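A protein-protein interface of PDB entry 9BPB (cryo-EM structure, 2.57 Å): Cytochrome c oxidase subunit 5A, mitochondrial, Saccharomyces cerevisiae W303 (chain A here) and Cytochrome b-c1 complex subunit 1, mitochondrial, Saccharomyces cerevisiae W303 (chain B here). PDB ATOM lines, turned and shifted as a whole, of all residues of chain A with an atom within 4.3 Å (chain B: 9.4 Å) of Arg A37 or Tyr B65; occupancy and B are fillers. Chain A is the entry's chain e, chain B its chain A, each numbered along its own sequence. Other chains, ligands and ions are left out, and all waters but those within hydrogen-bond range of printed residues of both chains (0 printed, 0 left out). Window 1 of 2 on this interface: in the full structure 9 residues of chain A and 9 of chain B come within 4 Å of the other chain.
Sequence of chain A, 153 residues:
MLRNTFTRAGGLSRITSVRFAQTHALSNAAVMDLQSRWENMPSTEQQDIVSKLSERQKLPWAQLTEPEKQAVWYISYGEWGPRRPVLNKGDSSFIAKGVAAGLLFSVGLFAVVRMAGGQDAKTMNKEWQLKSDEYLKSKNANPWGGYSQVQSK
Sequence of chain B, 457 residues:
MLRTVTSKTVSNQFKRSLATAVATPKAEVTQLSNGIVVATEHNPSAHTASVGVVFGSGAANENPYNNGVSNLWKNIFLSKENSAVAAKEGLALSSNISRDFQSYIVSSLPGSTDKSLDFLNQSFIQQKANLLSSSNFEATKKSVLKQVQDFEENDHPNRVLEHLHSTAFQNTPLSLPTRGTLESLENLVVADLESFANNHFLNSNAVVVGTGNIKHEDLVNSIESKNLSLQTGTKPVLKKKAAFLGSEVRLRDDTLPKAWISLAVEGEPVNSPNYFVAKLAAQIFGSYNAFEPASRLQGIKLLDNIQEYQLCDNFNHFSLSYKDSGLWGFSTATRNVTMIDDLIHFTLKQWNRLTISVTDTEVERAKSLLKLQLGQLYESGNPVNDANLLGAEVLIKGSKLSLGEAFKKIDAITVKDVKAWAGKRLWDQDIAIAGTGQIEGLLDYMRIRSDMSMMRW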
ATOM      1  N   ALA A  29       5.656  19.626 -24.872  1.00  0.00           N
ATOM      2  CA  ALA A  29       5.047  18.704 -25.825  1.00  0.00           C
ATOM      3  C   ALA A  29       3.998  17.821 -25.160  1.00  0.00           C
ATOM      4  O   ALA A  29       2.941  17.554 -25.743  1.00  0.00           O
ATOM      5  CB  ALA A  29       6.126  17.846 -26.486  1.00  0.00           C
ATOM      6  N   ALA A  30       4.276  17.350 -23.943  1.00  0.00           N
ATOM      7  CA  ALA A  30       3.376  16.402 -23.293  1.00  0.00           C
ATOM      8  C   ALA A  30       2.066  17.062 -22.875  1.00  0.00           C
ATOM      9  O   ALA A  30       0.982  16.543 -23.169  1.00  0.00           O
ATOM     10  CB  ALA A  30       4.069  15.769 -22.086  1.00  0.00           C
ATOM     11  N   MET A  32       0.525  19.991 -23.674  1.00  0.00           N
ATOM     12  CA  MET A  32      -0.331  20.706 -24.614  1.00  0.00           C
ATOM     13  C   MET A  32      -1.260  19.751 -25.352  1.00  0.00           C
ATOM     14  O   MET A  32      -0.829  18.711 -25.861  1.00  0.00           O
ATOM     15  CB  MET A  32       0.513  21.503 -25.608  1.00  0.00           C
ATOM     16  CG  MET A  32       0.884  22.887 -25.109  1.00  0.00           C
ATOM     17  SD  MET A  32       1.469  23.977 -26.418  1.00  0.00           S
ATOM     18  CE  MET A  32       1.629  25.519 -25.521  1.00  0.00           C
ATOM     19  N   ASP A  33      -2.541  20.120 -25.404  1.00  0.00           N
ATOM     20  CA  ASP A  33      -3.581  19.313 -26.043  1.00  0.00           C
ATOM     21  C   ASP A  33      -3.612  17.892 -25.485  1.00  0.00           C
ATOM     22  O   ASP A  33      -3.688  16.916 -26.232  1.00  0.00           O
ATOM     23  CB  ASP A  33      -3.412  19.299 -27.565  1.00  0.00           C
ATOM     24  CG  ASP A  33      -3.382  20.692 -28.159  1.00  0.00           C
ATOM     25  OD1 ASP A  33      -3.461  21.672 -27.388  1.00  0.00           O
ATOM     26  OD2 ASP A  33      -3.284  20.808 -29.399  1.00  0.00           O
ATOM     27  N   LEU A  34      -3.554  17.773 -24.161  1.00  0.00           N
ATOM     28  CA  LEU A  34      -3.693  16.472 -23.509  1.00  0.00           C
ATOM     29  C   LEU A  34      -5.157  16.164 -23.208  1.00  0.00           C
ATOM     30  O   LEU A  34      -5.535  15.800 -22.095  1.00  0.00           O
ATOM     31  CB  LEU A  34      -2.850  16.433 -22.238  1.00  0.00           C
ATOM     32  CG  LEU A  34      -2.501  15.061 -21.655  1.00  0.00           C
ATOM     33  CD1 LEU A  34      -1.295  14.459 -22.357  1.00  0.00           C
ATOM     34  CD2 LEU A  34      -2.262  15.162 -20.159  1.00  0.00           C
ATOM     35  N   GLN A  35      -5.996  16.318 -24.229  1.00  0.00           N
ATOM     36  CA  GLN A  35      -7.399  15.927 -24.185  1.00  0.00           C
ATOM     37  C   GLN A  35      -7.752  14.980 -25.318  1.00  0.00           C
ATOM     38  O   GLN A  35      -8.383  13.943 -25.085  1.00  0.00           O
ATOM     39  CB  GLN A  35      -8.299  17.171 -24.229  1.00  0.00           C
ATOM     40  CG  GLN A  35      -7.858  18.283 -23.295  1.00  0.00           C
ATOM     41  CD  GLN A  35      -8.651  19.558 -23.488  1.00  0.00           C
ATOM     42  OE1 GLN A  35      -9.584  19.607 -24.290  1.00  0.00           O
ATOM     43  NE2 GLN A  35      -8.283  20.602 -22.753  1.00  0.00           N
ATOM     44  N   SER A  36      -7.500  15.463 -26.529  1.00  0.00           N
ATOM     45  CA  SER A  36      -7.721  14.587 -27.689  1.00  0.00           C
ATOM     46  C   SER A  36      -6.605  13.547 -27.626  1.00  0.00           C
ATOM     47  O   SER A  36      -6.755  12.476 -28.238  1.00  0.00           O
ATOM     48  CB  SER A  36      -7.678  15.387 -28.937  1.00  0.00           C
ATOM     49  OG  SER A  36      -8.533  16.512 -28.835  1.00  0.00           O
ATOM     50  N   ARG A  37      -5.560  13.822 -26.841  1.00  0.00           N
ATOM     51  CA  ARG A  37      -4.404  12.893 -26.762  1.00  0.00           C
ATOM     52  C   ARG A  37      -4.568  11.911 -25.597  1.00  0.00           C
ATOM     53  O   ARG A  37      -3.671  11.067 -25.435  1.00  0.00           O
ATOM     54  CB  ARG A  37      -3.107  13.689 -26.606  1.00  0.00           C
ATOM     55  CG  ARG A  37      -2.683  14.432 -27.861  1.00  0.00           C
ATOM     56  CD  ARG A  37      -1.508  15.349 -27.594  1.00  0.00           C
ATOM     57  NE  ARG A  37      -0.272  14.667 -27.251  1.00  0.00           N
ATOM     58  CZ  ARG A  37       0.481  14.986 -26.208  1.00  0.00           C
ATOM     59  NH1 ARG A  37       1.714  14.525 -26.110  1.00  0.00           N
ATOM     60  NH2 ARG A  37      -0.001  15.791 -25.277  1.00  0.00           N
ATOM     61  N   TRP A  38      -5.647  12.006 -24.813  1.00  0.00           N
ATOM     62  CA  TRP A  38      -5.761  11.121 -23.612  1.00  0.00           C
ATOM     63  C   TRP A  38      -6.018   9.682 -24.061  1.00  0.00           C
ATOM     64  O   TRP A  38      -5.379   8.779 -23.508  1.00  0.00           O
ATOM     65  CB  TRP A  38      -6.842  11.631 -22.658  1.00  0.00           C
ATOM     66  CG  TRP A  38      -6.817  10.930 -21.336  1.00  0.00           C
ATOM     67  CD1 TRP A  38      -7.822  10.197 -20.777  1.00  0.00           C
ATOM     68  CD2 TRP A  38      -5.719  10.871 -20.409  1.00  0.00           C
ATOM     69  NE1 TRP A  38      -7.426   9.693 -19.570  1.00  0.00           N
ATOM     70  CE2 TRP A  38      -6.144  10.093 -19.314  1.00  0.00           C
ATOM     71  CE3 TRP A  38      -4.424  11.400 -20.392  1.00  0.00           C
ATOM     72  CZ2 TRP A  38      -5.322   9.831 -18.220  1.00  0.00           C
ATOM     73  CZ3 TRP A  38      -3.612  11.143 -19.311  1.00  0.00           C
ATOM     74  CH2 TRP A  38      -4.058  10.368 -18.241  1.00  0.00           C
ATOM     75  N   GLU A  39      -6.950   9.471 -24.970  1.00  0.00           N
ATOM     76  CA  GLU A  39      -7.287   8.217 -25.623  1.00  0.00           C
ATOM     77  C   GLU A  39      -6.277   7.933 -26.726  1.00  0.00           C
ATOM     78  O   GLU A  39      -5.614   8.841 -27.233  1.00  0.00           O
ATOM     79  CB  GLU A  39      -8.703   8.266 -26.195  1.00  0.00           C
ATOM     80  CG  GLU A  39      -9.771   8.653 -25.181  1.00  0.00           C
ATOM     81  CD  GLU A  39      -9.686   7.840 -23.902  1.00  0.00           C
ATOM     82  OE1 GLU A  39      -9.787   6.599 -23.978  1.00  0.00           O
ATOM     83  OE2 GLU A  39      -9.519   8.443 -22.820  1.00  0.00           O
ATOM     84  N   MET A  41      -3.602   6.475 -26.160  1.00  0.00           N
ATOM     85  CA  MET A  41      -2.320   6.820 -25.473  1.00  0.00           C
ATOM     86  C   MET A  41      -1.852   5.659 -24.582  1.00  0.00           C
ATOM     87  O   MET A  41      -2.629   5.261 -23.706  1.00  0.00           O
ATOM     88  CB  MET A  41      -2.563   8.056 -24.603  1.00  0.00           C
ATOM     89  CG  MET A  41      -1.490   8.377 -23.595  1.00  0.00           C
ATOM     90  SD  MET A  41      -1.890   9.964 -22.816  1.00  0.00           S
ATOM     91  CE  MET A  41      -0.253  10.549 -22.389  1.00  0.00           C
ATOM     92  N   GLU B  62       6.520   6.964 -31.782  1.00  0.00           N
ATOM     93  CA  GLU B  62       6.315   8.324 -31.314  1.00  0.00           C
ATOM     94  C   GLU B  62       4.997   8.887 -31.843  1.00  0.00           C
ATOM     95  O   GLU B  62       4.340   8.300 -32.705  1.00  0.00           O
ATOM     96  CB  GLU B  62       7.498   9.202 -31.716  1.00  0.00           C
ATOM     97  CG  GLU B  62       7.635   9.456 -33.197  1.00  0.00           C
ATOM     98  CD  GLU B  62       9.070   9.729 -33.589  1.00  0.00           C
ATOM     99  OE1 GLU B  62       9.961   9.524 -32.744  1.00  0.00           O
ATOM    100  OE2 GLU B  62       9.312  10.154 -34.738  1.00  0.00           O
ATOM    101  N   ASN B  63       4.606  10.030 -31.301  1.00  0.00           N
ATOM    102  CA  ASN B  63       3.324  10.662 -31.567  1.00  0.00           C
ATOM    103  C   ASN B  63       3.505  11.989 -32.304  1.00  0.00           C
ATOM    104  O   ASN B  63       4.626  12.491 -32.437  1.00  0.00           O
ATOM    105  CB  ASN B  63       2.560  10.858 -30.246  1.00  0.00           C
ATOM    106  CG  ASN B  63       3.197  11.887 -29.335  1.00  0.00           C
ATOM    107  OD1 ASN B  63       3.123  13.085 -29.586  1.00  0.00           O
ATOM    108  ND2 ASN B  63       3.818  11.420 -28.261  1.00  0.00           N
ATOM    109  N   PRO B  64       2.418  12.576 -32.827  1.00  0.00           N
ATOM    110  CA  PRO B  64       2.575  13.803 -33.631  1.00  0.00           C
ATOM    111  C   PRO B  64       3.122  14.999 -32.871  1.00  0.00           C
ATOM    112  O   PRO B  64       3.434  16.021 -33.494  1.00  0.00           O
ATOM    113  CB  PRO B  64       1.150  14.066 -34.133  1.00  0.00           C
ATOM    114  CG  PRO B  64       0.515  12.741 -34.158  1.00  0.00           C
ATOM    115  CD  PRO B  64       1.064  12.015 -32.971  1.00  0.00           C
ATOM    116  N   TYR B  65       3.244  14.922 -31.548  1.00  0.00           N
ATOM    117  CA  TYR B  65       3.679  16.113 -30.774  1.00  0.00           C
ATOM    118  C   TYR B  65       5.173  15.993 -30.462  1.00  0.00           C
ATOM    119  O   TYR B  65       5.815  17.034 -30.330  1.00  0.00           O
ATOM    120  CB  TYR B  65       2.764  16.309 -29.569  1.00  0.00           C
ATOM    121  CG  TYR B  65       1.353  16.667 -29.951  1.00  0.00           C
ATOM    122  CD1 TYR B  65       0.434  15.688 -30.284  1.00  0.00           C
ATOM    123  CD2 TYR B  65       0.941  17.987 -29.999  1.00  0.00           C
ATOM    124  CE1 TYR B  65      -0.860  16.011 -30.652  1.00  0.00           C
ATOM    125  CE2 TYR B  65      -0.350  18.326 -30.361  1.00  0.00           C
ATOM    126  CZ  TYR B  65      -1.255  17.335 -30.685  1.00  0.00           C
ATOM    127  OH  TYR B  65      -2.536  17.663 -31.044  1.00  0.00           O
ATOM    128  N   ASN B  66       5.700  14.780 -30.341  1.00  0.00           N
ATOM    129  CA  ASN B  66       7.135  14.587 -30.196  1.00  0.00           C
ATOM    130  C   ASN B  66       7.762  13.950 -31.429  1.00  0.00           C
ATOM    131  O   ASN B  66       8.862  13.397 -31.335  1.00  0.00           O
ATOM    132  CB  ASN B  66       7.445  13.751 -28.951  1.00  0.00           C
ATOM    133  CG  ASN B  66       6.908  12.337 -29.036  1.00  0.00           C
ATOM    134  OD1 ASN B  66       6.227  11.969 -29.990  1.00  0.00           O
ATOM    135  ND2 ASN B  66       7.227  11.528 -28.034  1.00  0.00           N
ATOM    136  N   ASN B  67       7.083  14.008 -32.571  1.00  0.00           N
ATOM    137  CA  ASN B  67       7.612  13.436 -33.800  1.00  0.00           C
ATOM    138  C   ASN B  67       8.942  14.086 -34.154  1.00  0.00           C
ATOM    139  O   ASN B  67       9.064  15.314 -34.185  1.00  0.00           O
ATOM    140  CB  ASN B  67       6.603  13.620 -34.935  1.00  0.00           C
ATOM    141  CG  ASN B  67       6.949  12.813 -36.169  1.00  0.00           C
ATOM    142  OD1 ASN B  67       7.953  12.105 -36.205  1.00  0.00           O
ATOM    143  ND2 ASN B  67       6.112  12.916 -37.191  1.00  0.00           N
ATOM    144  N   GLY B  68       9.941  13.254 -34.427  1.00  0.00           N
ATOM    145  CA  GLY B  68      11.288  13.723 -34.654  1.00  0.00           C
ATOM    146  C   GLY B  68      12.217  13.580 -33.470  1.00  0.00           C
ATOM    147  O   GLY B  68      13.367  14.026 -33.551  1.00  0.00           O
ATOM    148  N   VAL B  69      11.752  12.984 -32.371  1.00  0.00           N
ATOM    149  CA  VAL B  69      12.618  12.758 -31.217  1.00  0.00           C
ATOM    150  C   VAL B  69      13.677  11.705 -31.531  1.00  0.00           C
ATOM    151  O   VAL B  69      14.817  11.793 -31.060  1.00  0.00           O
ATOM    152  CB  VAL B  69      11.768  12.392 -29.982  1.00  0.00           C
ATOM    153  CG1 VAL B  69      11.022  11.092 -30.198  1.00  0.00           C
ATOM    154  CG2 VAL B  69      12.636  12.296 -28.748  1.00  0.00           C
ATOM    155  N   LEU B 176       3.916   8.400 -39.444  1.00  0.00           N
ATOM    156  CA  LEU B 176       4.720   9.526 -38.997  1.00  0.00           C
ATOM    157  C   LEU B 176       6.056   9.547 -39.738  1.00  0.00           C
ATOM    158  O   LEU B 176       6.754   8.530 -39.789  1.00  0.00           O
ATOM    159  CB  LEU B 176       4.954   9.458 -37.490  1.00  0.00           C
ATOM    160  CG  LEU B 176       3.849  10.058 -36.621  1.00  0.00           C
ATOM    161  CD1 LEU B 176       2.675   9.113 -36.483  1.00  0.00           C
ATOM    162  CD2 LEU B 176       4.400  10.426 -35.266  1.00  0.00           C
ATOM    163  N   GLY B 180      10.845  13.793 -38.916  1.00  0.00           N
ATOM    164  CA  GLY B 180      10.076  14.687 -38.076  1.00  0.00           C
ATOM    165  C   GLY B 180       9.651  15.935 -38.828  1.00  0.00           C
ATOM    166  O   GLY B 180      10.327  16.397 -39.757  1.00  0.00           O
ATOM    167  N   THR B 181       8.512  16.490 -38.425  1.00  0.00           N
ATOM    168  CA  THR B 181       7.995  17.684 -39.075  1.00  0.00           C
ATOM    169  C   THR B 181       8.705  18.935 -38.563  1.00  0.00           C
ATOM    170  O   THR B 181       9.329  18.933 -37.498  1.00  0.00           O
ATOM    171  CB  THR B 181       6.488  17.808 -38.854  1.00  0.00           C
ATOM    172  OG1 THR B 181       6.192  17.701 -37.457  1.00  0.00           O
ATOM    173  CG2 THR B 181       5.754  16.716 -39.604  1.00  0.00           C
ATOM    174  N   LEU B 182       8.617  20.007 -39.351  1.00  0.00           N
ATOM    175  CA  LEU B 182       9.240  21.270 -38.965  1.00  0.00           C
ATOM    176  C   LEU B 182       8.550  21.882 -37.754  1.00  0.00           C
ATOM    177  O   LEU B 182       9.207  22.445 -36.872  1.00  0.00           O
ATOM    178  CB  LEU B 182       9.215  22.244 -40.142  1.00  0.00           C
ATOM    179  CG  LEU B 182      10.298  23.319 -40.180  1.00  0.00           C
ATOM    180  CD1 LEU B 182      11.657  22.703 -40.456  1.00  0.00           C
ATOM    181  CD2 LEU B 182       9.958  24.363 -41.223  1.00  0.00           C
ATOM    182  N   GLU B 183       7.222  21.785 -37.695  1.00  0.00           N
ATOM    183  CA  GLU B 183       6.476  22.432 -36.622  1.00  0.00           C
ATOM    184  C   GLU B 183       6.672  21.721 -35.291  1.00  0.00           C
ATOM    185  O   GLU B 183       6.739  22.368 -34.240  1.00  0.00           O
ATOM    186  CB  GLU B 183       4.994  22.499 -36.988  1.00  0.00           C
ATOM    187  CG  GLU B 183       4.642  23.633 -37.951  1.00  0.00           C
ATOM    188  CD  GLU B 183       5.143  23.413 -39.368  1.00  0.00           C
ATOM    189  OE1 GLU B 183       5.664  22.319 -39.657  1.00  0.00           O
ATOM    190  OE2 GLU B 183       5.021  24.341 -40.198  1.00  0.00           O
ATOM    191  N   SER B 184       6.743  20.389 -35.309  1.00  0.00           N
ATOM    192  CA  SER B 184       6.852  19.647 -34.058  1.00  0.00           C
ATOM    193  C   SER B 184       8.275  19.680 -33.509  1.00  0.00           C
ATOM    194  O   SER B 184       8.465  19.700 -32.290  1.00  0.00           O
ATOM    195  CB  SER B 184       6.371  18.208 -34.250  1.00  0.00           C
ATOM    196  OG  SER B 184       7.270  17.450 -35.032  1.00  0.00           O
ATOM    197  N   LEU B 185       9.287  19.726 -34.382  1.00  0.00           N
ATOM    198  CA  LEU B 185      10.670  19.664 -33.911  1.00  0.00           C
ATOM    199  C   LEU B 185      11.049  20.884 -33.074  1.00  0.00           C
ATOM    200  O   LEU B 185      12.020  20.842 -32.311  1.00  0.00           O
ATOM    201  CB  LEU B 185      11.628  19.516 -35.091  1.00  0.00           C
ATOM    202  CG  LEU B 185      11.865  18.114 -35.641  1.00  0.00           C
ATOM    203  CD1 LEU B 185      12.629  18.187 -36.951  1.00  0.00           C
ATOM    204  CD2 LEU B 185      12.621  17.288 -34.625  1.00  0.00           C
ATOM    205  N   GLU B 186      10.304  21.981 -33.212  1.00  0.00           N
ATOM    206  CA  GLU B 186      10.609  23.183 -32.439  1.00  0.00           C
ATOM    207  C   GLU B 186      10.191  23.024 -30.983  1.00  0.00           C
ATOM    208  O   GLU B 186      10.856  23.540 -30.078  1.00  0.00           O
ATOM    209  CB  GLU B 186       9.926  24.394 -33.075  1.00  0.00           C
ATOM    210  CG  GLU B 186      10.518  25.753 -32.694  1.00  0.00           C
ATOM    211  CD  GLU B 186      10.053  26.249 -31.335  1.00  0.00           C
ATOM    212  OE1 GLU B 186       8.981  25.812 -30.876  1.00  0.00           O
ATOM    213  OE2 GLU B 186      10.745  27.096 -30.736  1.00  0.00           O
ATOM    214  N   ASN B 187       9.087  22.315 -30.736  1.00  0.00           N
ATOM    215  CA  ASN B 187       8.518  22.262 -29.394  1.00  0.00           C
ATOM    216  C   ASN B 187       9.292  21.339 -28.461  1.00  0.00           C
ATOM    217  O   ASN B 187       9.101  21.396 -27.242  1.00  0.00           O
ATOM    218  CB  ASN B 187       7.056  21.835 -29.469  1.00  0.00           C
ATOM    219  CG  ASN B 187       6.219  22.808 -30.266  1.00  0.00           C
ATOM    220  OD1 ASN B 187       5.515  22.429 -31.200  1.00  0.00           O
ATOM    221  ND2 ASN B 187       6.289  24.076 -29.891  1.00  0.00           N
ATOM    222  N   LEU B 188      10.158  20.484 -28.999  1.00  0.00           N
ATOM    223  CA  LEU B 188      10.876  19.552 -28.140  1.00  0.00           C
ATOM    224  C   LEU B 188      11.823  20.276 -27.196  1.00  0.00           C
ATOM    225  O   LEU B 188      12.347  21.348 -27.508  1.00  0.00           O
ATOM    226  CB  LEU B 188      11.658  18.523 -28.959  1.00  0.00           C
ATOM    227  CG  LEU B 188      10.960  17.322 -29.604  1.00  0.00           C
ATOM    228  CD1 LEU B 188      10.106  17.682 -30.765  1.00  0.00           C
ATOM    229  CD2 LEU B 188      12.005  16.324 -30.033  1.00  0.00           C
ATOM    230  N   VAL B 189      12.012  19.684 -26.017  1.00  0.00           N
ATOM    231  CA  VAL B 189      13.058  20.060 -25.078  1.00  0.00           C
ATOM    232  C   VAL B 189      13.773  18.782 -24.657  1.00  0.00           C
ATOM    233  O   VAL B 189      13.445  17.686 -25.111  1.00  0.00           O
ATOM    234  CB  VAL B 189      12.515  20.819 -23.847  1.00  0.00           C
ATOM    235  CG1 VAL B 189      11.969  22.171 -24.255  1.00  0.00           C
ATOM    236  CG2 VAL B 189      11.440  20.002 -23.135  1.00  0.00           C
ATOM    237  N   ASP B 192      11.613  15.799 -23.281  1.00  0.00           N
ATOM    238  CA  ASP B 192      11.045  14.826 -24.207  1.00  0.00           C
ATOM    239  C   ASP B 192      12.056  13.739 -24.554  1.00  0.00           C
ATOM    240  O   ASP B 192      11.712  12.550 -24.602  1.00  0.00           O
ATOM    241  CB  ASP B 192      10.564  15.532 -25.473  1.00  0.00           C
ATOM    242  CG  ASP B 192       9.374  16.435 -25.220  1.00  0.00           C
ATOM    243  OD1 ASP B 192       8.578  16.129 -24.306  1.00  0.00           O
ATOM    244  OD2 ASP B 192       9.235  17.452 -25.929  1.00  0.00           O
ATOM    245  N   SER B 195      12.520  11.421 -21.567  1.00  0.00           N
ATOM    246  CA  SER B 195      11.324  10.600 -21.414  1.00  0.00           C
ATOM    247  C   SER B 195      11.309   9.458 -22.420  1.00  0.00           C
ATOM    248  O   SER B 195      11.016   8.310 -22.063  1.00  0.00           O
ATOM    249  CB  SER B 195      10.077  11.467 -21.566  1.00  0.00           C
ATOM    250  OG  SER B 195       8.911  10.671 -21.656  1.00  0.00           O
ATOM    251  N   LYS B 239      -1.964   1.309 -28.613  1.00  0.00           N
ATOM    252  CA  LYS B 239      -3.403   0.958 -28.506  1.00  0.00           C
ATOM    253  C   LYS B 239      -4.009   0.720 -29.889  1.00  0.00           C
ATOM    254  O   LYS B 239      -4.999  -0.017 -29.967  1.00  0.00           O
ATOM    255  CB  LYS B 239      -4.172   2.063 -27.778  1.00  0.00           C
ATOM    256  CG  LYS B 239      -3.965   2.119 -26.272  1.00  0.00           C
ATOM    257  CD  LYS B 239      -4.928   3.060 -25.588  1.00  0.00           C
ATOM    258  CE  LYS B 239      -4.996   2.855 -24.091  1.00  0.00           C
ATOM    259  NZ  LYS B 239      -5.930   3.814 -23.455  1.00  0.00           N
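N of Tyr B65 lies within hydrogen-bond range of OD1 of Asn B63, 2.7 Å away. O of Ala A30 is in hydrogen-bond range of NH2 of Arg A37 (2.4 Å). The backbone carbonyl oxygen (O) of Met A32 lies within hydrogen-bond range of the guanidinium group (NH2) of Arg A37, at 3.1 Å. O of Ala A29 lies within hydrogen-bond range of NH1 of Arg A37.
Printed residues of chain B that touch a printed residue of chain A: Tyr B65, Asp B192 and Lys B239. Hydrophobic or aromatic side chains of chain A that line the printed part of chain B: Ala A29. Among the printed residues, no Asp or Glu carboxylate lies within 4 Å of a Lys or Arg side-chain nitrogen of the other chain.
Ala A29 touches Tyr B65. Asp B192 touches Ala A29 (OD2 to CB, 3.2 Å). Asp A33 touches Tyr B65. Arg A37 touches Tyr B65. O of Met A41 touches CE of Lys B239, 3.4 Å away.
Of the printed residues of chain B, Arg A37 touches Tyr B65. Tyr B65 touches three residues of chain A. No residue of chain B comes within 4 Å of Ala A30. No residue of chain B comes within 4 Å of Ser A36. Of the printed residues of chain B, Ala A29 touches Tyr B65 (3.9 Å) and Asp B192 (3.2 Å). Of the printed residues of chain A, Asp B192 touches Ala A29 (3.2 Å). Of the printed residues of chain B, Asp A33 touches Tyr B65. Of the printed residues of chain B, Met A41 touches Lys B239. Of the printed residues of chain A, Lys B239 touches Met A41. The nearest printed residue of chain A that does not touch Tyr B65 is Met A32 (4.5 Å). The nearest printed residue of chain B that does not touch Asp A33 is Asn B63 (8.5 Å).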
